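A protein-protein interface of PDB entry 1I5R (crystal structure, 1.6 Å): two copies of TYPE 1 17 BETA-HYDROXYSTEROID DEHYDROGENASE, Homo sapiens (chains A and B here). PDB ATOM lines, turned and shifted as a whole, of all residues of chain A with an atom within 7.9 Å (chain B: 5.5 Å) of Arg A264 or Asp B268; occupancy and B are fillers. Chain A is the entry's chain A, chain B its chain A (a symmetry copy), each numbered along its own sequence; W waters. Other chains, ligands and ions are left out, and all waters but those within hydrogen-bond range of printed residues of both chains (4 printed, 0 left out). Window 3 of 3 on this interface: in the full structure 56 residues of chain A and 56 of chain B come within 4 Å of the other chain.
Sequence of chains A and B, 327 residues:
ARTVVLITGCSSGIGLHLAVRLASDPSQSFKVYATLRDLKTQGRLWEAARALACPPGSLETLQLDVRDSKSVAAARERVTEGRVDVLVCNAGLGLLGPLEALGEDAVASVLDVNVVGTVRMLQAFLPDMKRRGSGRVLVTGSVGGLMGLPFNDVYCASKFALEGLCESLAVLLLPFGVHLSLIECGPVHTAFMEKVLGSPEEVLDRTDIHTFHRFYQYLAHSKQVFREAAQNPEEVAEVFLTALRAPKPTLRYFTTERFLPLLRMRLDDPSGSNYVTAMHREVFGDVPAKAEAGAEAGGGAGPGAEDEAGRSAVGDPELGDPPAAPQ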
ATOM      1  N   LEU A 146      33.979  18.549  19.571  1.00  0.00           N
ATOM      2  CA  LEU A 146      33.079  17.582  20.159  1.00  0.00           C
ATOM      3  C   LEU A 146      32.902  16.342  19.312  1.00  0.00           C
ATOM      4  O   LEU A 146      32.449  15.334  19.822  1.00  0.00           O
ATOM      5  CB  LEU A 146      31.717  18.254  20.324  1.00  0.00           C
ATOM      6  CG  LEU A 146      31.733  19.575  21.107  1.00  0.00           C
ATOM      7  CD1 LEU A 146      30.322  20.132  21.153  1.00  0.00           C
ATOM      8  CD2 LEU A 146      32.274  19.317  22.502  1.00  0.00           C
ATOM      9  N   MET A 147      33.285  16.465  18.053  1.00  0.00           N
ATOM     10  CA  MET A 147      33.166  15.314  17.163  1.00  0.00           C
ATOM     11  C   MET A 147      34.166  15.514  16.039  1.00  0.00           C
ATOM     12  O   MET A 147      34.436  16.653  15.672  1.00  0.00           O
ATOM     13  CB  MET A 147      31.738  15.236  16.666  1.00  0.00           C
ATOM     14  CG  MET A 147      31.409  16.427  15.769  1.00  0.00           C
ATOM     15  SD  MET A 147      29.655  16.352  15.396  1.00  0.00           S
ATOM     16  CE  MET A 147      29.629  17.234  13.837  1.00  0.00           C
ATOM     17  N   PHE A 259      23.878  20.178  15.750  1.00  0.00           N
ATOM     18  CA  PHE A 259      24.769  19.034  15.802  1.00  0.00           C
ATOM     19  C   PHE A 259      24.638  18.170  17.037  1.00  0.00           C
ATOM     20  O   PHE A 259      25.219  17.078  17.062  1.00  0.00           O
ATOM     21  CB  PHE A 259      26.231  19.519  15.704  1.00  0.00           C
ATOM     22  CG  PHE A 259      26.411  20.376  14.480  1.00  0.00           C
ATOM     23  CD1 PHE A 259      26.462  19.803  13.222  1.00  0.00           C
ATOM     24  CD2 PHE A 259      26.485  21.756  14.607  1.00  0.00           C
ATOM     25  CE1 PHE A 259      26.612  20.600  12.100  1.00  0.00           C
ATOM     26  CE2 PHE A 259      26.627  22.547  13.485  1.00  0.00           C
ATOM     27  CZ  PHE A 259      26.712  21.970  12.231  1.00  0.00           C
ATOM     28  N   LEU A 260      23.769  18.543  17.971  1.00  0.00           N
ATOM     29  CA  LEU A 260      23.528  17.773  19.187  1.00  0.00           C
ATOM     30  C   LEU A 260      23.217  16.323  18.858  1.00  0.00           C
ATOM     31  O   LEU A 260      23.856  15.422  19.406  1.00  0.00           O
ATOM     32  CB  LEU A 260      22.465  18.418  20.067  1.00  0.00           C
ATOM     33  CG  LEU A 260      22.868  19.532  21.030  1.00  0.00           C
ATOM     34  CD1 LEU A 260      23.534  18.962  22.277  1.00  0.00           C
ATOM     35  CD2 LEU A 260      23.806  20.542  20.389  1.00  0.00           C
ATOM     36  N   PRO A 261      22.314  16.065  17.922  1.00  0.00           N
ATOM     37  CA  PRO A 261      22.004  14.712  17.489  1.00  0.00           C
ATOM     38  C   PRO A 261      23.231  13.910  17.102  1.00  0.00           C
ATOM     39  O   PRO A 261      23.455  12.827  17.670  1.00  0.00           O
ATOM     40  CB  PRO A 261      21.065  14.913  16.304  1.00  0.00           C
ATOM     41  CG  PRO A 261      20.401  16.217  16.584  1.00  0.00           C
ATOM     42  CD  PRO A 261      21.450  17.069  17.250  1.00  0.00           C
ATOM     43  N   LEU A 262      24.068  14.397  16.179  1.00  0.00           N
ATOM     44  CA  LEU A 262      25.291  13.703  15.790  1.00  0.00           C
ATOM     45  C   LEU A 262      26.164  13.480  17.027  1.00  0.00           C
ATOM     46  O   LEU A 262      26.799  12.444  17.197  1.00  0.00           O
ATOM     47  CB  LEU A 262      26.112  14.463  14.757  1.00  0.00           C
ATOM     48  CG  LEU A 262      25.684  14.419  13.295  1.00  0.00           C
ATOM     49  CD1 LEU A 262      26.413  15.502  12.509  1.00  0.00           C
ATOM     50  CD2 LEU A 262      25.980  13.053  12.687  1.00  0.00           C
ATOM     51  N   LEU A 263      26.211  14.499  17.883  1.00  0.00           N
ATOM     52  CA  LEU A 263      26.937  14.443  19.133  1.00  0.00           C
ATOM     53  C   LEU A 263      26.414  13.388  20.088  1.00  0.00           C
ATOM     54  O   LEU A 263      27.199  12.673  20.708  1.00  0.00           O
ATOM     55  CB  LEU A 263      26.877  15.820  19.817  1.00  0.00           C
ATOM     56  CG  LEU A 263      27.634  16.878  18.995  1.00  0.00           C
ATOM     57  CD1 LEU A 263      27.448  18.271  19.564  1.00  0.00           C
ATOM     58  CD2 LEU A 263      29.112  16.501  18.961  1.00  0.00           C
ATOM     59  N   ARG A 264      25.091  13.284  20.215  1.00  0.00           N
ATOM     60  CA  ARG A 264      24.458  12.299  21.083  1.00  0.00           C
ATOM     61  C   ARG A 264      24.899  10.901  20.677  1.00  0.00           C
ATOM     62  O   ARG A 264      25.184  10.015  21.479  1.00  0.00           O
ATOM     63  CB  ARG A 264      22.939  12.420  21.059  1.00  0.00           C
ATOM     64  CG  ARG A 264      22.402  13.704  21.657  1.00  0.00           C
ATOM     65  CD  ARG A 264      22.513  13.732  23.173  1.00  0.00           C
ATOM     66  NE  ARG A 264      21.892  14.929  23.726  1.00  0.00           N
ATOM     67  CZ  ARG A 264      21.703  15.182  25.012  1.00  0.00           C
ATOM     68  NH1 ARG A 264      22.078  14.325  25.949  1.00  0.00           N
ATOM     69  NH2 ARG A 264      21.117  16.324  25.354  1.00  0.00           N
ATOM     70  N   MET A 265      24.990  10.689  19.374  1.00  0.00           N
ATOM     71  CA  MET A 265      25.462   9.459  18.771  1.00  0.00           C
ATOM     72  C   MET A 265      26.833   9.036  19.269  1.00  0.00           C
ATOM     73  O   MET A 265      27.076   7.831  19.391  1.00  0.00           O
ATOM     74  CB  MET A 265      25.457   9.659  17.260  1.00  0.00           C
ATOM     75  CG  MET A 265      26.062   8.523  16.456  1.00  0.00           C
ATOM     76  SD  MET A 265      25.784   8.849  14.707  1.00  0.00           S
ATOM     77  CE  MET A 265      23.996   8.858  14.617  1.00  0.00           C
ATOM     78  N   ARG A 266      27.750   9.959  19.566  1.00  0.00           N
ATOM     79  CA  ARG A 266      29.045   9.583  20.110  1.00  0.00           C
ATOM     80  C   ARG A 266      28.948   8.905  21.464  1.00  0.00           C
ATOM     81  O   ARG A 266      29.717   7.972  21.697  1.00  0.00           O
ATOM     82  CB  ARG A 266      29.982  10.793  20.250  1.00  0.00           C
ATOM     83  CG  ARG A 266      30.394  11.338  18.901  1.00  0.00           C
ATOM     84  CD  ARG A 266      31.251  12.594  19.017  1.00  0.00           C
ATOM     85  NE  ARG A 266      32.643  12.219  19.219  1.00  0.00           N
ATOM     86  CZ  ARG A 266      33.234  12.049  20.381  1.00  0.00           C
ATOM     87  NH1 ARG A 266      32.571  12.260  21.520  1.00  0.00           N
ATOM     88  NH2 ARG A 266      34.512  11.668  20.488  1.00  0.00           N
ATOM     89  N   LEU A 267      28.101   9.371  22.385  1.00  0.00           N
ATOM     90  CA  LEU A 267      28.046   8.701  23.688  1.00  0.00           C
ATOM     91  C   LEU A 267      27.137   7.485  23.650  1.00  0.00           C
ATOM     92  O   LEU A 267      27.387   6.473  24.314  1.00  0.00           O
ATOM     93  CB  LEU A 267      27.567   9.575  24.830  1.00  0.00           C
ATOM     94  CG  LEU A 267      27.455   8.862  26.184  1.00  0.00           C
ATOM     95  CD1 LEU A 267      28.641   9.193  27.068  1.00  0.00           C
ATOM     96  CD2 LEU A 267      26.134   9.124  26.878  1.00  0.00           C
ATOM     97  N   ASP A 268      26.136   7.527  22.768  1.00  0.00           N
ATOM     98  CA  ASP A 268      25.265   6.362  22.591  1.00  0.00           C
ATOM     99  C   ASP A 268      26.155   5.158  22.267  1.00  0.00           C
ATOM    100  O   ASP A 268      25.890   4.027  22.643  1.00  0.00           O
ATOM    101  CB  ASP A 268      24.220   6.597  21.515  1.00  0.00           C
ATOM    102  CG  ASP A 268      23.132   7.563  21.940  1.00  0.00           C
ATOM    103  OD1 ASP A 268      22.569   7.363  23.039  1.00  0.00           O
ATOM    104  OD2 ASP A 268      22.820   8.514  21.199  1.00  0.00           O
ATOM    105  N   ASP A 269      27.242   5.433  21.540  1.00  0.00           N
ATOM    106  CA  ASP A 269      28.222   4.427  21.209  1.00  0.00           C
ATOM    107  C   ASP A 269      29.648   4.845  21.525  1.00  0.00           C
ATOM    108  O   ASP A 269      30.365   5.399  20.681  1.00  0.00           O
ATOM    109  CB  ASP A 269      28.035   4.100  19.722  1.00  0.00           C
ATOM    110  CG  ASP A 269      29.073   3.106  19.240  1.00  0.00           C
ATOM    111  OD1 ASP A 269      29.654   2.431  20.118  1.00  0.00           O
ATOM    112  OD2 ASP A 269      29.298   3.002  18.025  1.00  0.00           O
ATOM    113  N   PRO A 270      30.131   4.521  22.716  1.00  0.00           N
ATOM    114  CA  PRO A 270      31.480   4.826  23.156  1.00  0.00           C
ATOM    115  C   PRO A 270      32.552   4.157  22.318  1.00  0.00           C
ATOM    116  O   PRO A 270      33.639   4.725  22.195  1.00  0.00           O
ATOM    117  CB  PRO A 270      31.559   4.340  24.595  1.00  0.00           C
ATOM    118  CG  PRO A 270      30.147   4.193  25.041  1.00  0.00           C
ATOM    119  CD  PRO A 270      29.359   3.864  23.804  1.00  0.00           C
ATOM    120  N   ASN A 274      29.468   4.093  15.656  1.00  0.00           N
ATOM    121  CA  ASN A 274      28.256   4.718  15.147  1.00  0.00           C
ATOM    122  C   ASN A 274      28.576   6.094  14.581  1.00  0.00           C
ATOM    123  O   ASN A 274      28.176   6.413  13.476  1.00  0.00           O
ATOM    124  CB  ASN A 274      27.199   4.864  16.231  1.00  0.00           C
ATOM    125  CG  ASN A 274      26.563   3.514  16.544  1.00  0.00           C
ATOM    126  OD1 ASN A 274      26.884   2.520  15.893  1.00  0.00           O
ATOM    127  ND2 ASN A 274      25.685   3.532  17.529  1.00  0.00           N
ATOM    128  N   TYR A 275      29.320   6.855  15.376  1.00  0.00           N
ATOM    129  CA  TYR A 275      29.667   8.189  14.900  1.00  0.00           C
ATOM    130  C   TYR A 275      30.480   8.103  13.623  1.00  0.00           C
ATOM    131  O   TYR A 275      30.186   8.790  12.648  1.00  0.00           O
ATOM    132  CB  TYR A 275      30.405   8.956  16.010  1.00  0.00           C
ATOM    133  CG  TYR A 275      30.815  10.292  15.420  1.00  0.00           C
ATOM    134  CD1 TYR A 275      29.899  11.323  15.321  1.00  0.00           C
ATOM    135  CD2 TYR A 275      32.103  10.455  14.934  1.00  0.00           C
ATOM    136  CE1 TYR A 275      30.264  12.537  14.767  1.00  0.00           C
ATOM    137  CE2 TYR A 275      32.470  11.660  14.356  1.00  0.00           C
ATOM    138  CZ  TYR A 275      31.552  12.680  14.285  1.00  0.00           C
ATOM    139  OH  TYR A 275      31.898  13.878  13.715  1.00  0.00           O
ATOM    140  N   ARG B 264      29.236   8.656  30.547  1.00  0.00           N
ATOM    141  CA  ARG B 264      27.856   8.752  30.088  1.00  0.00           C
ATOM    142  C   ARG B 264      27.264  10.084  30.525  1.00  0.00           C
ATOM    143  O   ARG B 264      26.544  10.778  29.812  1.00  0.00           O
ATOM    144  CB  ARG B 264      27.012   7.589  30.593  1.00  0.00           C
ATOM    145  CG  ARG B 264      27.400   6.238  30.026  1.00  0.00           C
ATOM    146  CD  ARG B 264      26.990   6.078  28.571  1.00  0.00           C
ATOM    147  NE  ARG B 264      27.278   4.735  28.085  1.00  0.00           N
ATOM    148  CZ  ARG B 264      26.918   4.239  26.911  1.00  0.00           C
ATOM    149  NH1 ARG B 264      26.230   4.958  26.038  1.00  0.00           N
ATOM    150  NH2 ARG B 264      27.258   2.989  26.620  1.00  0.00           N
ATOM    151  N   MET B 265      27.598  10.483  31.741  1.00  0.00           N
ATOM    152  CA  MET B 265      27.210  11.750  32.327  1.00  0.00           C
ATOM    153  C   MET B 265      27.591  12.947  31.473  1.00  0.00           C
ATOM    154  O   MET B 265      26.841  13.927  31.454  1.00  0.00           O
ATOM    155  CB  MET B 265      27.847  11.829  33.710  1.00  0.00           C
ATOM    156  CG  MET B 265      27.675  13.157  34.426  1.00  0.00           C
ATOM    157  SD  MET B 265      28.311  12.989  36.101  1.00  0.00           S
ATOM    158  CE  MET B 265      27.243  11.719  36.773  1.00  0.00           C
ATOM    159  N   ARG B 266      28.720  12.926  30.759  1.00  0.00           N
ATOM    160  CA  ARG B 266      29.071  14.029  29.881  1.00  0.00           C
ATOM    161  C   ARG B 266      28.082  14.227  28.748  1.00  0.00           C
ATOM    162  O   ARG B 266      27.814  15.382  28.413  1.00  0.00           O
ATOM    163  CB  ARG B 266      30.469  13.849  29.265  1.00  0.00           C
ATOM    164  CG  ARG B 266      31.557  13.966  30.309  1.00  0.00           C
ATOM    165  CD  ARG B 266      32.944  13.701  29.736  1.00  0.00           C
ATOM    166  NE  ARG B 266      33.470  14.922  29.144  1.00  0.00           N
ATOM    167  CZ  ARG B 266      33.331  15.291  27.890  1.00  0.00           C
ATOM    168  NH1 ARG B 266      32.697  14.508  27.015  1.00  0.00           N
ATOM    169  NH2 ARG B 266      33.814  16.449  27.424  1.00  0.00           N
ATOM    170  N   LEU B 267      27.588  13.169  28.099  1.00  0.00           N
ATOM    171  CA  LEU B 267      26.647  13.400  27.000  1.00  0.00           C
ATOM    172  C   LEU B 267      25.229  13.589  27.511  1.00  0.00           C
ATOM    173  O   LEU B 267      24.442  14.365  26.956  1.00  0.00           O
ATOM    174  CB  LEU B 267      26.598  12.294  25.964  1.00  0.00           C
ATOM    175  CG  LEU B 267      25.574  12.504  24.842  1.00  0.00           C
ATOM    176  CD1 LEU B 267      26.253  12.997  23.578  1.00  0.00           C
ATOM    177  CD2 LEU B 267      24.716  11.282  24.591  1.00  0.00           C
ATOM    178  N   ASP B 268      24.930  12.974  28.657  1.00  0.00           N
ATOM    179  CA  ASP B 268      23.619  13.176  29.278  1.00  0.00           C
ATOM    180  C   ASP B 268      23.416  14.683  29.463  1.00  0.00           C
ATOM    181  O   ASP B 268      22.321  15.214  29.363  1.00  0.00           O
ATOM    182  CB  ASP B 268      23.495  12.425  30.592  1.00  0.00           C
ATOM    183  CG  ASP B 268      23.373  10.925  30.414  1.00  0.00           C
ATOM    184  OD1 ASP B 268      22.520  10.500  29.603  1.00  0.00           O
ATOM    185  OD2 ASP B 268      24.103  10.159  31.070  1.00  0.00           O
ATOM    186  N   ASP B 269      24.524  15.377  29.743  1.00  0.00           N
ATOM    187  CA  ASP B 269      24.520  16.814  29.876  1.00  0.00           C
ATOM    188  C   ASP B 269      25.595  17.499  29.050  1.00  0.00           C
ATOM    189  O   ASP B 269      26.713  17.754  29.521  1.00  0.00           O
ATOM    190  CB  ASP B 269      24.661  17.120  31.372  1.00  0.00           C
ATOM    191  CG  ASP B 269      24.751  18.612  31.624  1.00  0.00           C
ATOM    192  OD1 ASP B 269      24.339  19.361  30.712  1.00  0.00           O
ATOM    193  OD2 ASP B 269      25.216  19.021  32.699  1.00  0.00           O
ATOM    194  N   PRO B 270      25.270  17.893  27.827  1.00  0.00           N
ATOM    195  CA  PRO B 270      26.177  18.583  26.928  1.00  0.00           C
ATOM    196  C   PRO B 270      26.638  19.929  27.454  1.00  0.00           C
ATOM    197  O   PRO B 270      27.756  20.334  27.128  1.00  0.00           O
ATOM    198  CB  PRO B 270      25.405  18.763  25.630  1.00  0.00           C
ATOM    199  CG  PRO B 270      24.281  17.792  25.700  1.00  0.00           C
ATOM    200  CD  PRO B 270      23.966  17.633  27.162  1.00  0.00           C
ATOM    201  N   ASN B 274      26.880  18.738  34.695  1.00  0.00           N
ATOM    202  CA  ASN B 274      26.745  17.519  35.478  1.00  0.00           C
ATOM    203  C   ASN B 274      28.112  16.887  35.700  1.00  0.00           C
ATOM    204  O   ASN B 274      28.456  16.543  36.817  1.00  0.00           O
ATOM    205  CB  ASN B 274      25.839  16.506  34.793  1.00  0.00           C
ATOM    206  CG  ASN B 274      24.379  16.932  34.907  1.00  0.00           C
ATOM    207  OD1 ASN B 274      24.082  17.936  35.553  1.00  0.00           O
ATOM    208  ND2 ASN B 274      23.525  16.150  34.274  1.00  0.00           N
HETATM  209  O   HOH W   1      26.046   1.941  24.379  1.00  0.00           O
HETATM  210  O   HOH W   2      21.660  11.921  27.401  1.00  0.00           O
HETATM  211  O   HOH W   3      20.357  16.502  27.996  1.00  0.00           O
HETATM  212  O   HOH W   4      23.776   6.095  25.170  1.00  0.00           O
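O of Leu A267 lies within hydrogen-bond range of NH1 of Arg B264, 2.6 Å away. O of Leu B267 is in hydrogen-bond range of NH1 of Arg A264 (2.6 Å).
Pro B270 touches Leu A260 (CG to CD1, 3.7 Å). Leu B267 touches Leu A263 (CD1 to O, 3.0 Å). Arg A264 touches Asp B268. Arg A264 touches Pro B270 (NH2 to CG, 3.5 Å). Leu A267 touches Leu B267 (CB to CB, 3.1 Å). Arg B264 touches Asp A268. Pro A270 touches Arg B264.
Arg A264 touches three residues of chain B. Asp B268 touches one residue of chain A. Of the printed residues of chain B, Pro A270 touches Arg B264 (3.5 Å). Printed residues of chain B within 4 Å of Leu A267: Arg B264 (2.6 Å) and Leu B267 (3.1 Å).
Of the 16 printed residues of chain A, 6 touch a printed residue of chain B. Hydrophobic or aromatic side chains of chain A within 4 Å of the printed part of chain B: Leu A260, Leu A267 and Pro A270. Printed residues of chain B that touch a printed residue of chain A: Arg B264, Leu B267, Asp B268 and Pro B270. Hydrophobic or aromatic side chains of chain B that line the printed part of chain A: Leu B267 and Pro B270. Among the printed residues, 9 pairs touch across the chains.
Arg A264 touches Leu B267, and with the chains exchanged Leu A267 touches Arg B264. Arg A264 touches Asp B268, and with the chains exchanged Asp A268 touches Arg B264. Arg A264 touches Pro B270, and with the chains exchanged Pro A270 touches Arg B264. Leu A267 touches its own counterpart, Leu B267.
Water W3 lies within hydrogen-bond range of O of Asp B268 and NH2 of Arg A264. Water W1 bridges O of Asp A268 and NH2 of Arg B264. Water W4 bridges OD1 of Asp A268 (2.8 Å) and NH1 of Arg B264 (2.8 Å). Water W2 bridges OD1 of Asp B268 (2.8 Å) and NH1 of Arg A264 (2.8 Å).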
